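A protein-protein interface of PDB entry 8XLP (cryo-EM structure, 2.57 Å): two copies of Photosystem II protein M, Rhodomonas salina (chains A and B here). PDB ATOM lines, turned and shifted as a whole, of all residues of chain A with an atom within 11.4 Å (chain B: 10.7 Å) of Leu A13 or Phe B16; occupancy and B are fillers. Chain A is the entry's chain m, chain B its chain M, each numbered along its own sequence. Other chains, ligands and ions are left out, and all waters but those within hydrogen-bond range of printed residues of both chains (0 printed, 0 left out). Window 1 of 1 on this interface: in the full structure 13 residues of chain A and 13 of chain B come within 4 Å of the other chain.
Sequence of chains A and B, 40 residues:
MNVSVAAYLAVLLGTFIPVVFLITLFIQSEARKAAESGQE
OG1 of Thr A24 sits close to OG1 of Thr B24 (2.3 Å).
The backbone carbonyl oxygen (O) of Val A20 sits at hydrogen-bond distance from the side-chain hydroxyl (OG1) of Thr A24, at 2.8 Å.
The backbone carbonyl oxygen (O) of Val B20 lies within hydrogen-bond range of the side-chain hydroxyl (OG1) of Thr B24 (2.7 Å).
O of Val A5 touches CG2 of Val B5, at 3.6 Å.
Val A5 touches Tyr B8.
Val B5 touches Tyr A8.
CD2 of Leu B9 touches CD2 of Leu A9 (3.7 Å).
Leu A13 touches Phe B16 (CD2 to CD2, 3.5 Å).
Val A20 touches Val B20 (CG2 to CG1, 3.8 Å).
Of the printed residues of chain B, Val A5 touches Val B5 and Tyr B8.
Leu A9 touches just one residue of chain B: Leu B9 (3.7 Å).
Leu A12 touches none of the printed residues of chain B.
Printed residues of chain B within 4 Å of Leu A13: Phe B16.
No residue of chain B comes within 4 Å of Thr A15.
No residue of chain B comes within 4 Å of Ile A17.
Of the printed residues of chain B, Val A20 touches Val B20 (3.8 Å).
Leu A22 touches none of the printed residues of chain B.
Of the printed residues of chain B, Thr A24 touches Thr B24.
Printed residues of chain A within 4 Å of Tyr B8: Val A5.
Leu B12 touches none of the printed residues of chain A.
No residue of chain A comes within 4 Å of Gly B14.
Of the printed residues of chain A, Phe B16 touches Leu A13.
No residue of chain A comes within 4 Å of Pro B18.
No residue of chain A comes within 4 Å of Val B19.
The nearest printed residue of chain B that does not touch Tyr A8 is Leu B9 (4.4 Å).
Of the 19 printed residues of chain B, 6 touch a printed residue of chain A.
Hydrophobic or aromatic side chains of chain B that line the printed part of chain A: Val B5, Tyr B8, Leu B9, Phe B16 and Val B20.
Of the 20 printed residues of chain A, 6 touch a printed residue of chain B.
Hydrophobic or aromatic side chains of chain A within 4 Å of the printed part of chain B: Val A5, Tyr A8, Leu A9, Leu A13 and Val A20.
Among the printed residues, 7 pairs touch across the chains.
Among the printed residues, no Asp or Glu carboxylate lies within 4 Å of a Lys or Arg side-chain nitrogen of the other chain.
Val A5 touches its own counterpart, Val B5.
Leu A9 touches its own counterpart, Leu B9.
Leu A13 touches Phe B16, but with the chains exchanged Phe A16 does not touch Leu B13 (4.01 Å).
Val A20 touches its own counterpart, Val B20.
Of the 7 pairs that touch across the chains among the printed residues, 6 have their exchanged pair printed and touching as well.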
ATOM      1  N   SER A   4      29.667   7.772 -29.666  1.00  0.00           N
ATOM      2  CA  SER A   4      28.407   7.481 -29.000  1.00  0.00           C
ATOM      3  C   SER A   4      28.617   6.673 -27.723  1.00  0.00           C
ATOM      4  O   SER A   4      29.565   5.894 -27.594  1.00  0.00           O
ATOM      5  CB  SER A   4      27.473   6.724 -29.945  1.00  0.00           C
ATOM      6  OG  SER A   4      26.254   6.393 -29.302  1.00  0.00           O
ATOM      7  N   VAL A   5      27.709   6.884 -26.766  1.00  0.00           N
ATOM      8  CA  VAL A   5      27.650   6.054 -25.565  1.00  0.00           C
ATOM      9  C   VAL A   5      27.369   4.607 -25.942  1.00  0.00           C
ATOM     10  O   VAL A   5      27.967   3.667 -25.395  1.00  0.00           O
ATOM     11  CB  VAL A   5      26.574   6.606 -24.607  1.00  0.00           C
ATOM     12  CG1 VAL A   5      26.413   5.718 -23.380  1.00  0.00           C
ATOM     13  CG2 VAL A   5      26.886   8.048 -24.219  1.00  0.00           C
ATOM     14  N   ALA A   6      26.447   4.414 -26.888  1.00  0.00           N
ATOM     15  CA  ALA A   6      26.052   3.080 -27.313  1.00  0.00           C
ATOM     16  C   ALA A   6      27.218   2.299 -27.901  1.00  0.00           C
ATOM     17  O   ALA A   6      27.271   1.078 -27.758  1.00  0.00           O
ATOM     18  CB  ALA A   6      24.914   3.179 -28.329  1.00  0.00           C
ATOM     19  N   ALA A   7      28.167   2.973 -28.548  1.00  0.00           N
ATOM     20  CA  ALA A   7      29.282   2.250 -29.153  1.00  0.00           C
ATOM     21  C   ALA A   7      30.173   1.613 -28.089  1.00  0.00           C
ATOM     22  O   ALA A   7      30.498   0.418 -28.167  1.00  0.00           O
ATOM     23  CB  ALA A   7      30.079   3.192 -30.053  1.00  0.00           C
ATOM     24  N   TYR A   8      30.561   2.391 -27.072  1.00  0.00           N
ATOM     25  CA  TYR A   8      31.336   1.836 -25.966  1.00  0.00           C
ATOM     26  C   TYR A   8      30.552   0.761 -25.227  1.00  0.00           C
ATOM     27  O   TYR A   8      31.111  -0.283 -24.860  1.00  0.00           O
ATOM     28  CB  TYR A   8      31.744   2.935 -24.986  1.00  0.00           C
ATOM     29  CG  TYR A   8      32.724   3.953 -25.517  1.00  0.00           C
ATOM     30  CD1 TYR A   8      32.283   5.083 -26.189  1.00  0.00           C
ATOM     31  CD2 TYR A   8      34.089   3.797 -25.320  1.00  0.00           C
ATOM     32  CE1 TYR A   8      33.173   6.023 -26.665  1.00  0.00           C
ATOM     33  CE2 TYR A   8      34.990   4.732 -25.794  1.00  0.00           C
ATOM     34  CZ  TYR A   8      34.525   5.843 -26.466  1.00  0.00           C
ATOM     35  OH  TYR A   8      35.414   6.779 -26.941  1.00  0.00           O
ATOM     36  N   LEU A   9      29.260   1.008 -24.982  1.00  0.00           N
ATOM     37  CA  LEU A   9      28.440   0.018 -24.287  1.00  0.00           C
ATOM     38  C   LEU A   9      28.395  -1.296 -25.057  1.00  0.00           C
ATOM     39  O   LEU A   9      28.579  -2.374 -24.480  1.00  0.00           O
ATOM     40  CB  LEU A   9      27.027   0.565 -24.070  1.00  0.00           C
ATOM     41  CG  LEU A   9      26.813   1.500 -22.879  1.00  0.00           C
ATOM     42  CD1 LEU A   9      25.422   2.110 -22.928  1.00  0.00           C
ATOM     43  CD2 LEU A   9      27.019   0.750 -21.573  1.00  0.00           C
ATOM     44  N   ALA A  10      28.175  -1.218 -26.371  1.00  0.00           N
ATOM     45  CA  ALA A  10      28.123  -2.413 -27.203  1.00  0.00           C
ATOM     46  C   ALA A  10      29.444  -3.166 -27.167  1.00  0.00           C
ATOM     47  O   ALA A  10      29.465  -4.385 -26.965  1.00  0.00           O
ATOM     48  CB  ALA A  10      27.754  -2.039 -28.638  1.00  0.00           C
ATOM     49  N   VAL A  11      30.562  -2.454 -27.346  1.00  0.00           N
ATOM     50  CA  VAL A  11      31.861  -3.126 -27.376  1.00  0.00           C
ATOM     51  C   VAL A  11      32.134  -3.825 -26.047  1.00  0.00           C
ATOM     52  O   VAL A  11      32.440  -5.026 -26.006  1.00  0.00           O
ATOM     53  CB  VAL A  11      32.979  -2.130 -27.730  1.00  0.00           C
ATOM     54  CG1 VAL A  11      34.343  -2.783 -27.566  1.00  0.00           C
ATOM     55  CG2 VAL A  11      32.805  -1.624 -29.153  1.00  0.00           C
ATOM     56  N   LEU A  12      31.979  -3.095 -24.936  1.00  0.00           N
ATOM     57  CA  LEU A  12      32.308  -3.662 -23.630  1.00  0.00           C
ATOM     58  C   LEU A  12      31.390  -4.825 -23.272  1.00  0.00           C
ATOM     59  O   LEU A  12      31.857  -5.860 -22.779  1.00  0.00           O
ATOM     60  CB  LEU A  12      32.251  -2.578 -22.553  1.00  0.00           C
ATOM     61  CG  LEU A  12      33.551  -1.822 -22.249  1.00  0.00           C
ATOM     62  CD1 LEU A  12      34.684  -2.791 -21.946  1.00  0.00           C
ATOM     63  CD2 LEU A  12      33.941  -0.879 -23.378  1.00  0.00           C
ATOM     64  N   LEU A  13      30.083  -4.691 -23.525  1.00  0.00           N
ATOM     65  CA  LEU A  13      29.157  -5.751 -23.139  1.00  0.00           C
ATOM     66  C   LEU A  13      29.296  -6.976 -24.035  1.00  0.00           C
ATOM     67  O   LEU A  13      29.306  -8.111 -23.542  1.00  0.00           O
ATOM     68  CB  LEU A  13      27.721  -5.227 -23.155  1.00  0.00           C
ATOM     69  CG  LEU A  13      27.360  -4.291 -21.997  1.00  0.00           C
ATOM     70  CD1 LEU A  13      25.975  -3.713 -22.223  1.00  0.00           C
ATOM     71  CD2 LEU A  13      27.437  -4.991 -20.647  1.00  0.00           C
ATOM     72  N   GLY A  14      29.404  -6.775 -25.353  1.00  0.00           N
ATOM     73  CA  GLY A  14      29.616  -7.891 -26.253  1.00  0.00           C
ATOM     74  C   GLY A  14      30.958  -8.564 -26.078  1.00  0.00           C
ATOM     75  O   GLY A  14      31.137  -9.696 -26.539  1.00  0.00           O
ATOM     76  N   THR A  15      31.911  -7.891 -25.430  1.00  0.00           N
ATOM     77  CA  THR A  15      33.125  -8.584 -25.025  1.00  0.00           C
ATOM     78  C   THR A  15      32.910  -9.368 -23.735  1.00  0.00           C
ATOM     79  O   THR A  15      33.243 -10.554 -23.659  1.00  0.00           O
ATOM     80  CB  THR A  15      34.271  -7.585 -24.852  1.00  0.00           C
ATOM     81  OG1 THR A  15      34.368  -6.759 -26.017  1.00  0.00           O
ATOM     82  CG2 THR A  15      35.587  -8.320 -24.645  1.00  0.00           C
ATOM     83  N   PHE A  16      32.333  -8.725 -22.717  1.00  0.00           N
ATOM     84  CA  PHE A  16      32.340  -9.307 -21.377  1.00  0.00           C
ATOM     85  C   PHE A  16      31.341 -10.450 -21.232  1.00  0.00           C
ATOM     86  O   PHE A  16      31.658 -11.471 -20.608  1.00  0.00           O
ATOM     87  CB  PHE A  16      32.077  -8.220 -20.336  1.00  0.00           C
ATOM     88  CG  PHE A  16      33.240  -7.293 -20.129  1.00  0.00           C
ATOM     89  CD1 PHE A  16      34.513  -7.656 -20.539  1.00  0.00           C
ATOM     90  CD2 PHE A  16      33.065  -6.060 -19.526  1.00  0.00           C
ATOM     91  CE1 PHE A  16      35.587  -6.809 -20.352  1.00  0.00           C
ATOM     92  CE2 PHE A  16      34.136  -5.207 -19.334  1.00  0.00           C
ATOM     93  CZ  PHE A  16      35.399  -5.583 -19.749  1.00  0.00           C
ATOM     94  N   ILE A  17      30.127 -10.302 -21.775  1.00  0.00           N
ATOM     95  CA  ILE A  17      29.081 -11.305 -21.539  1.00  0.00           C
ATOM     96  C   ILE A  17      29.451 -12.683 -22.083  1.00  0.00           C
ATOM     97  O   ILE A  17      29.337 -13.669 -21.333  1.00  0.00           O
ATOM     98  CB  ILE A  17      27.727 -10.792 -22.061  1.00  0.00           C
ATOM     99  CG1 ILE A  17      27.281  -9.560 -21.270  1.00  0.00           C
ATOM    100  CG2 ILE A  17      26.674 -11.888 -21.990  1.00  0.00           C
ATOM    101  CD1 ILE A  17      25.946  -9.000 -21.712  1.00  0.00           C
ATOM    102  N   PRO A  18      29.886 -12.840 -23.345  1.00  0.00           N
ATOM    103  CA  PRO A  18      30.363 -14.172 -23.760  1.00  0.00           C
ATOM    104  C   PRO A  18      31.567 -14.647 -22.966  1.00  0.00           C
ATOM    105  O   PRO A  18      31.692 -15.848 -22.696  1.00  0.00           O
ATOM    106  CB  PRO A  18      30.698 -13.980 -25.246  1.00  0.00           C
ATOM    107  CG  PRO A  18      29.913 -12.797 -25.666  1.00  0.00           C
ATOM    108  CD  PRO A  18      29.922 -11.895 -24.478  1.00  0.00           C
ATOM    109  N   VAL A  19      32.451 -13.727 -22.572  1.00  0.00           N
ATOM    110  CA  VAL A  19      33.638 -14.103 -21.810  1.00  0.00           C
ATOM    111  C   VAL A  19      33.242 -14.675 -20.454  1.00  0.00           C
ATOM    112  O   VAL A  19      33.738 -15.731 -20.039  1.00  0.00           O
ATOM    113  CB  VAL A  19      34.589 -12.898 -21.666  1.00  0.00           C
ATOM    114  CG1 VAL A  19      35.486 -13.057 -20.446  1.00  0.00           C
ATOM    115  CG2 VAL A  19      35.433 -12.745 -22.919  1.00  0.00           C
ATOM    116  N   VAL A  20      32.332 -13.997 -19.748  1.00  0.00           N
ATOM    117  CA  VAL A  20      31.919 -14.501 -18.443  1.00  0.00           C
ATOM    118  C   VAL A  20      31.099 -15.776 -18.591  1.00  0.00           C
ATOM    119  O   VAL A  20      31.160 -16.656 -17.726  1.00  0.00           O
ATOM    120  CB  VAL A  20      31.171 -13.422 -17.632  1.00  0.00           C
ATOM    121  CG1 VAL A  20      32.063 -12.206 -17.415  1.00  0.00           C
ATOM    122  CG2 VAL A  20      29.867 -13.020 -18.296  1.00  0.00           C
ATOM    123  N   PHE A  21      30.343 -15.918 -19.686  1.00  0.00           N
ATOM    124  CA  PHE A  21      29.635 -17.173 -19.934  1.00  0.00           C
ATOM    125  C   PHE A  21      30.612 -18.336 -20.090  1.00  0.00           C
ATOM    126  O   PHE A  21      30.441 -19.399 -19.476  1.00  0.00           O
ATOM    127  CB  PHE A  21      28.753 -17.037 -21.176  1.00  0.00           C
ATOM    128  CG  PHE A  21      28.358 -18.352 -21.789  1.00  0.00           C
ATOM    129  CD1 PHE A  21      27.441 -19.178 -21.160  1.00  0.00           C
ATOM    130  CD2 PHE A  21      28.896 -18.757 -23.001  1.00  0.00           C
ATOM    131  CE1 PHE A  21      27.075 -20.386 -21.722  1.00  0.00           C
ATOM    132  CE2 PHE A  21      28.532 -19.965 -23.569  1.00  0.00           C
ATOM    133  CZ  PHE A  21      27.620 -20.780 -22.928  1.00  0.00           C
ATOM    134  N   LEU A  22      31.653 -18.144 -20.905  1.00  0.00           N
ATOM    135  CA  LEU A  22      32.649 -19.192 -21.110  1.00  0.00           C
ATOM    136  C   LEU A  22      33.401 -19.503 -19.821  1.00  0.00           C
ATOM    137  O   LEU A  22      33.666 -20.673 -19.516  1.00  0.00           O
ATOM    138  CB  LEU A  22      33.623 -18.775 -22.213  1.00  0.00           C
ATOM    139  CG  LEU A  22      33.042 -18.658 -23.621  1.00  0.00           C
ATOM    140  CD1 LEU A  22      33.819 -17.637 -24.433  1.00  0.00           C
ATOM    141  CD2 LEU A  22      33.044 -20.009 -24.317  1.00  0.00           C
ATOM    142  N   THR A  24      32.317 -19.088 -16.720  1.00  0.00           N
ATOM    143  CA  THR A  24      31.402 -19.802 -15.835  1.00  0.00           C
ATOM    144  C   THR A  24      31.269 -21.263 -16.240  1.00  0.00           C
ATOM    145  O   THR A  24      31.290 -22.158 -15.385  1.00  0.00           O
ATOM    146  CB  THR A  24      30.033 -19.121 -15.843  1.00  0.00           C
ATOM    147  OG1 THR A  24      30.164 -17.769 -15.388  1.00  0.00           O
ATOM    148  CG2 THR A  24      29.056 -19.863 -14.944  1.00  0.00           C
ATOM    149  N   VAL B   5      29.152   8.574 -21.389  1.00  0.00           N
ATOM    150  CA  VAL B   5      29.170   7.115 -21.455  1.00  0.00           C
ATOM    151  C   VAL B   5      29.738   6.498 -20.180  1.00  0.00           C
ATOM    152  O   VAL B   5      29.399   5.360 -19.830  1.00  0.00           O
ATOM    153  CB  VAL B   5      29.959   6.673 -22.708  1.00  0.00           C
ATOM    154  CG1 VAL B   5      31.374   7.234 -22.679  1.00  0.00           C
ATOM    155  CG2 VAL B   5      29.971   5.157 -22.856  1.00  0.00           C
ATOM    156  N   TYR B   8      26.956   5.443 -17.646  1.00  0.00           N
ATOM    157  CA  TYR B   8      26.265   4.233 -18.083  1.00  0.00           C
ATOM    158  C   TYR B   8      27.151   3.007 -17.915  1.00  0.00           C
ATOM    159  O   TYR B   8      26.684   1.950 -17.473  1.00  0.00           O
ATOM    160  CB  TYR B   8      25.827   4.369 -19.543  1.00  0.00           C
ATOM    161  CG  TYR B   8      24.721   5.371 -19.785  1.00  0.00           C
ATOM    162  CD1 TYR B   8      25.002   6.723 -19.934  1.00  0.00           C
ATOM    163  CD2 TYR B   8      23.396   4.962 -19.880  1.00  0.00           C
ATOM    164  CE1 TYR B   8      23.994   7.641 -20.161  1.00  0.00           C
ATOM    165  CE2 TYR B   8      22.382   5.873 -20.108  1.00  0.00           C
ATOM    166  CZ  TYR B   8      22.686   7.211 -20.248  1.00  0.00           C
ATOM    167  OH  TYR B   8      21.681   8.122 -20.474  1.00  0.00           O
ATOM    168  N   LEU B   9      28.433   3.133 -18.268  1.00  0.00           N
ATOM    169  CA  LEU B   9      29.366   2.027 -18.086  1.00  0.00           C
ATOM    170  C   LEU B   9      29.506   1.665 -16.617  1.00  0.00           C
ATOM    171  O   LEU B   9      29.530   0.482 -16.266  1.00  0.00           O
ATOM    172  CB  LEU B   9      30.729   2.384 -18.680  1.00  0.00           C
ATOM    173  CG  LEU B   9      30.842   2.343 -20.205  1.00  0.00           C
ATOM    174  CD1 LEU B   9      32.204   2.844 -20.654  1.00  0.00           C
ATOM    175  CD2 LEU B   9      30.597   0.932 -20.711  1.00  0.00           C
ATOM    176  N   ALA B  10      29.580   2.670 -15.742  1.00  0.00           N
ATOM    177  CA  ALA B  10      29.681   2.408 -14.312  1.00  0.00           C
ATOM    178  C   ALA B  10      28.472   1.629 -13.816  1.00  0.00           C
ATOM    179  O   ALA B  10      28.620   0.589 -13.164  1.00  0.00           O
ATOM    180  CB  ALA B  10      29.826   3.724 -13.547  1.00  0.00           C
ATOM    181  N   VAL B  11      27.266   2.089 -14.161  1.00  0.00           N
ATOM    182  CA  VAL B  11      26.056   1.418 -13.689  1.00  0.00           C
ATOM    183  C   VAL B  11      25.992  -0.011 -14.221  1.00  0.00           C
ATOM    184  O   VAL B  11      25.839  -0.973 -13.455  1.00  0.00           O
ATOM    185  CB  VAL B  11      24.804   2.223 -14.081  1.00  0.00           C
ATOM    186  CG1 VAL B  11      23.544   1.465 -13.691  1.00  0.00           C
ATOM    187  CG2 VAL B  11      24.828   3.593 -13.422  1.00  0.00           C
ATOM    188  N   LEU B  12      26.158  -0.175 -15.539  1.00  0.00           N
ATOM    189  CA  LEU B  12      25.994  -1.492 -16.148  1.00  0.00           C
ATOM    190  C   LEU B  12      27.068  -2.471 -15.682  1.00  0.00           C
ATOM    191  O   LEU B  12      26.760  -3.628 -15.373  1.00  0.00           O
ATOM    192  CB  LEU B  12      25.997  -1.375 -17.672  1.00  0.00           C
ATOM    193  CG  LEU B  12      24.642  -1.182 -18.365  1.00  0.00           C
ATOM    194  CD1 LEU B  12      23.657  -2.259 -17.936  1.00  0.00           C
ATOM    195  CD2 LEU B  12      24.062   0.200 -18.112  1.00  0.00           C
ATOM    196  N   LEU B  13      28.328  -2.033 -15.609  1.00  0.00           N
ATOM    197  CA  LEU B  13      29.400  -2.939 -15.216  1.00  0.00           C
ATOM    198  C   LEU B  13      29.343  -3.265 -13.729  1.00  0.00           C
ATOM    199  O   LEU B  13      29.506  -4.428 -13.341  1.00  0.00           O
ATOM    200  CB  LEU B  13      30.757  -2.343 -15.592  1.00  0.00           C
ATOM    201  CG  LEU B  13      31.016  -2.163 -17.093  1.00  0.00           C
ATOM    202  CD1 LEU B  13      32.488  -1.875 -17.333  1.00  0.00           C
ATOM    203  CD2 LEU B  13      30.565  -3.367 -17.909  1.00  0.00           C
ATOM    204  N   GLY B  14      29.109  -2.261 -12.875  1.00  0.00           N
ATOM    205  CA  GLY B  14      28.958  -2.529 -11.459  1.00  0.00           C
ATOM    206  C   GLY B  14      27.729  -3.341 -11.124  1.00  0.00           C
ATOM    207  O   GLY B  14      27.652  -3.905 -10.027  1.00  0.00           O
ATOM    208  N   THR B  15      26.759  -3.407 -12.039  1.00  0.00           N
ATOM    209  CA  THR B  15      25.674  -4.364 -11.869  1.00  0.00           C
ATOM    210  C   THR B  15      26.087  -5.756 -12.338  1.00  0.00           C
ATOM    211  O   THR B  15      25.925  -6.737 -11.606  1.00  0.00           O
ATOM    212  CB  THR B  15      24.433  -3.895 -12.628  1.00  0.00           C
ATOM    213  OG1 THR B  15      24.106  -2.558 -12.234  1.00  0.00           O
ATOM    214  CG2 THR B  15      23.254  -4.810 -12.333  1.00  0.00           C
ATOM    215  N   PHE B  16      26.642  -5.856 -13.548  1.00  0.00           N
ATOM    216  CA  PHE B  16      26.824  -7.156 -14.186  1.00  0.00           C
ATOM    217  C   PHE B  16      27.976  -7.957 -13.587  1.00  0.00           C
ATOM    218  O   PHE B  16      27.834  -9.167 -13.374  1.00  0.00           O
ATOM    219  CB  PHE B  16      27.030  -6.972 -15.689  1.00  0.00           C
ATOM    220  CG  PHE B  16      25.782  -6.574 -16.425  1.00  0.00           C
ATOM    221  CD1 PHE B  16      24.534  -6.763 -15.852  1.00  0.00           C
ATOM    222  CD2 PHE B  16      25.855  -6.015 -17.686  1.00  0.00           C
ATOM    223  CE1 PHE B  16      23.385  -6.399 -16.526  1.00  0.00           C
ATOM    224  CE2 PHE B  16      24.710  -5.650 -18.367  1.00  0.00           C
ATOM    225  CZ  PHE B  16      23.473  -5.842 -17.785  1.00  0.00           C
ATOM    226  N   ILE B  17      29.123  -7.319 -13.324  1.00  0.00           N
ATOM    227  CA  ILE B  17      30.301  -8.068 -12.871  1.00  0.00           C
ATOM    228  C   ILE B  17      30.066  -8.781 -11.541  1.00  0.00           C
ATOM    229  O   ILE B  17      30.359  -9.986 -11.454  1.00  0.00           O
ATOM    230  CB  ILE B  17      31.536  -7.150 -12.853  1.00  0.00           C
ATOM    231  CG1 ILE B  17      31.880  -6.684 -14.269  1.00  0.00           C
ATOM    232  CG2 ILE B  17      32.721  -7.859 -12.215  1.00  0.00           C
ATOM    233  CD1 ILE B  17      33.088  -5.775 -14.335  1.00  0.00           C
ATOM    234  N   PRO B  18      29.552  -8.130 -10.483  1.00  0.00           N
ATOM    235  CA  PRO B  18      29.198  -8.912  -9.287  1.00  0.00           C
ATOM    236  C   PRO B  18      28.125  -9.953  -9.554  1.00  0.00           C
ATOM    237  O   PRO B  18      28.167 -11.043  -8.972  1.00  0.00           O
ATOM    238  CB  PRO B  18      28.722  -7.842  -8.295  1.00  0.00           C
ATOM    239  CG  PRO B  18      29.331  -6.581  -8.769  1.00  0.00           C
ATOM    240  CD  PRO B  18      29.324  -6.689 -10.255  1.00  0.00           C
ATOM    241  N   VAL B  19      27.169  -9.649 -10.437  1.00  0.00           N
ATOM    242  CA  VAL B  19      26.099 -10.595 -10.739  1.00  0.00           C
ATOM    243  C   VAL B  19      26.662 -11.844 -11.406  1.00  0.00           C
ATOM    244  O   VAL B  19      26.330 -12.973 -11.024  1.00  0.00           O
ATOM    245  CB  VAL B  19      25.014  -9.924 -11.604  1.00  0.00           C
ATOM    246  CG1 VAL B  19      24.240 -10.961 -12.406  1.00  0.00           C
ATOM    247  CG2 VAL B  19      24.059  -9.134 -10.724  1.00  0.00           C
ATOM    248  N   VAL B  20      27.534 -11.664 -12.403  1.00  0.00           N
ATOM    249  CA  VAL B  20      28.102 -12.829 -13.074  1.00  0.00           C
ATOM    250  C   VAL B  20      29.053 -13.575 -12.146  1.00  0.00           C
ATOM    251  O   VAL B  20      29.159 -14.803 -12.225  1.00  0.00           O
ATOM    252  CB  VAL B  20      28.778 -12.441 -14.406  1.00  0.00           C
ATOM    253  CG1 VAL B  20      27.770 -11.792 -15.345  1.00  0.00           C
ATOM    254  CG2 VAL B  20      29.974 -11.531 -14.185  1.00  0.00           C
ATOM    255  N   PHE B  21      29.737 -12.867 -11.240  1.00  0.00           N
ATOM    256  CA  PHE B  21      30.567 -13.546 -10.246  1.00  0.00           C
ATOM    257  C   PHE B  21      29.726 -14.447  -9.346  1.00  0.00           C
ATOM    258  O   PHE B  21      30.065 -15.617  -9.120  1.00  0.00           O
ATOM    259  CB  PHE B  21      31.333 -12.513  -9.417  1.00  0.00           C
ATOM    260  CG  PHE B  21      31.834 -13.038  -8.101  1.00  0.00           C
ATOM    261  CD1 PHE B  21      32.899 -13.923  -8.053  1.00  0.00           C
ATOM    262  CD2 PHE B  21      31.247 -12.639  -6.910  1.00  0.00           C
ATOM    263  CE1 PHE B  21      33.363 -14.406  -6.844  1.00  0.00           C
ATOM    264  CE2 PHE B  21      31.708 -13.118  -5.698  1.00  0.00           C
ATOM    265  CZ  PHE B  21      32.768 -14.003  -5.665  1.00  0.00           C
ATOM    266  N   LEU B  22      28.613 -13.914  -8.831  1.00  0.00           N
ATOM    267  CA  LEU B  22      27.733 -14.699  -7.969  1.00  0.00           C
ATOM    268  C   LEU B  22      27.121 -15.873  -8.723  1.00  0.00           C
ATOM    269  O   LEU B  22      27.014 -16.980  -8.181  1.00  0.00           O
ATOM    270  CB  LEU B  22      26.638 -13.805  -7.390  1.00  0.00           C
ATOM    271  CG  LEU B  22      27.087 -12.717  -6.413  1.00  0.00           C
ATOM    272  CD1 LEU B  22      26.128 -11.542  -6.458  1.00  0.00           C
ATOM    273  CD2 LEU B  22      27.186 -13.273  -5.002  1.00  0.00           C
ATOM    274  N   ILE B  23      26.706 -15.646  -9.972  1.00  0.00           N
ATOM    275  CA  ILE B  23      26.113 -16.714 -10.770  1.00  0.00           C
ATOM    276  C   ILE B  23      27.135 -17.812 -11.044  1.00  0.00           C
ATOM    277  O   ILE B  23      26.821 -19.004 -10.952  1.00  0.00           O
ATOM    278  CB  ILE B  23      25.522 -16.136 -12.071  1.00  0.00           C
ATOM    279  CG1 ILE B  23      24.274 -15.306 -11.762  1.00  0.00           C
ATOM    280  CG2 ILE B  23      25.185 -17.241 -13.055  1.00  0.00           C
ATOM    281  CD1 ILE B  23      23.635 -14.683 -12.983  1.00  0.00           C
ATOM    282  N   THR B  24      28.375 -17.431 -11.369  1.00  0.00           N
ATOM    283  CA  THR B  24      29.427 -18.416 -11.595  1.00  0.00           C
ATOM    284  C   THR B  24      29.703 -19.226 -10.336  1.00  0.00           C
ATOM    285  O   THR B  24      29.851 -20.453 -10.397  1.00  0.00           O
ATOM    286  CB  THR B  24      30.702 -17.718 -12.069  1.00  0.00           C
ATOM    287  OG1 THR B  24      30.427 -16.972 -13.261  1.00  0.00           O
ATOM    288  CG2 THR B  24      31.797 -18.735 -12.354  1.00  0.00           C
ATOM    289  N   LEU B  25      29.767 -18.557  -9.182  1.00  0.00           N
ATOM    290  CA  LEU B  25      30.018 -19.265  -7.931  1.00  0.00           C
ATOM    291  C   LEU B  25      28.887 -20.236  -7.601  1.00  0.00           C
ATOM    292  O   LEU B  25      29.136 -21.380  -7.197  1.00  0.00           O
ATOM    293  CB  LEU B  25      30.214 -18.256  -6.801  1.00  0.00           C
ATOM    294  CG  LEU B  25      30.806 -18.785  -5.499  1.00  0.00           C
ATOM    295  CD1 LEU B  25      32.119 -19.490  -5.765  1.00  0.00           C
ATOM    296  CD2 LEU B  25      31.000 -17.640  -4.532  1.00  0.00           C
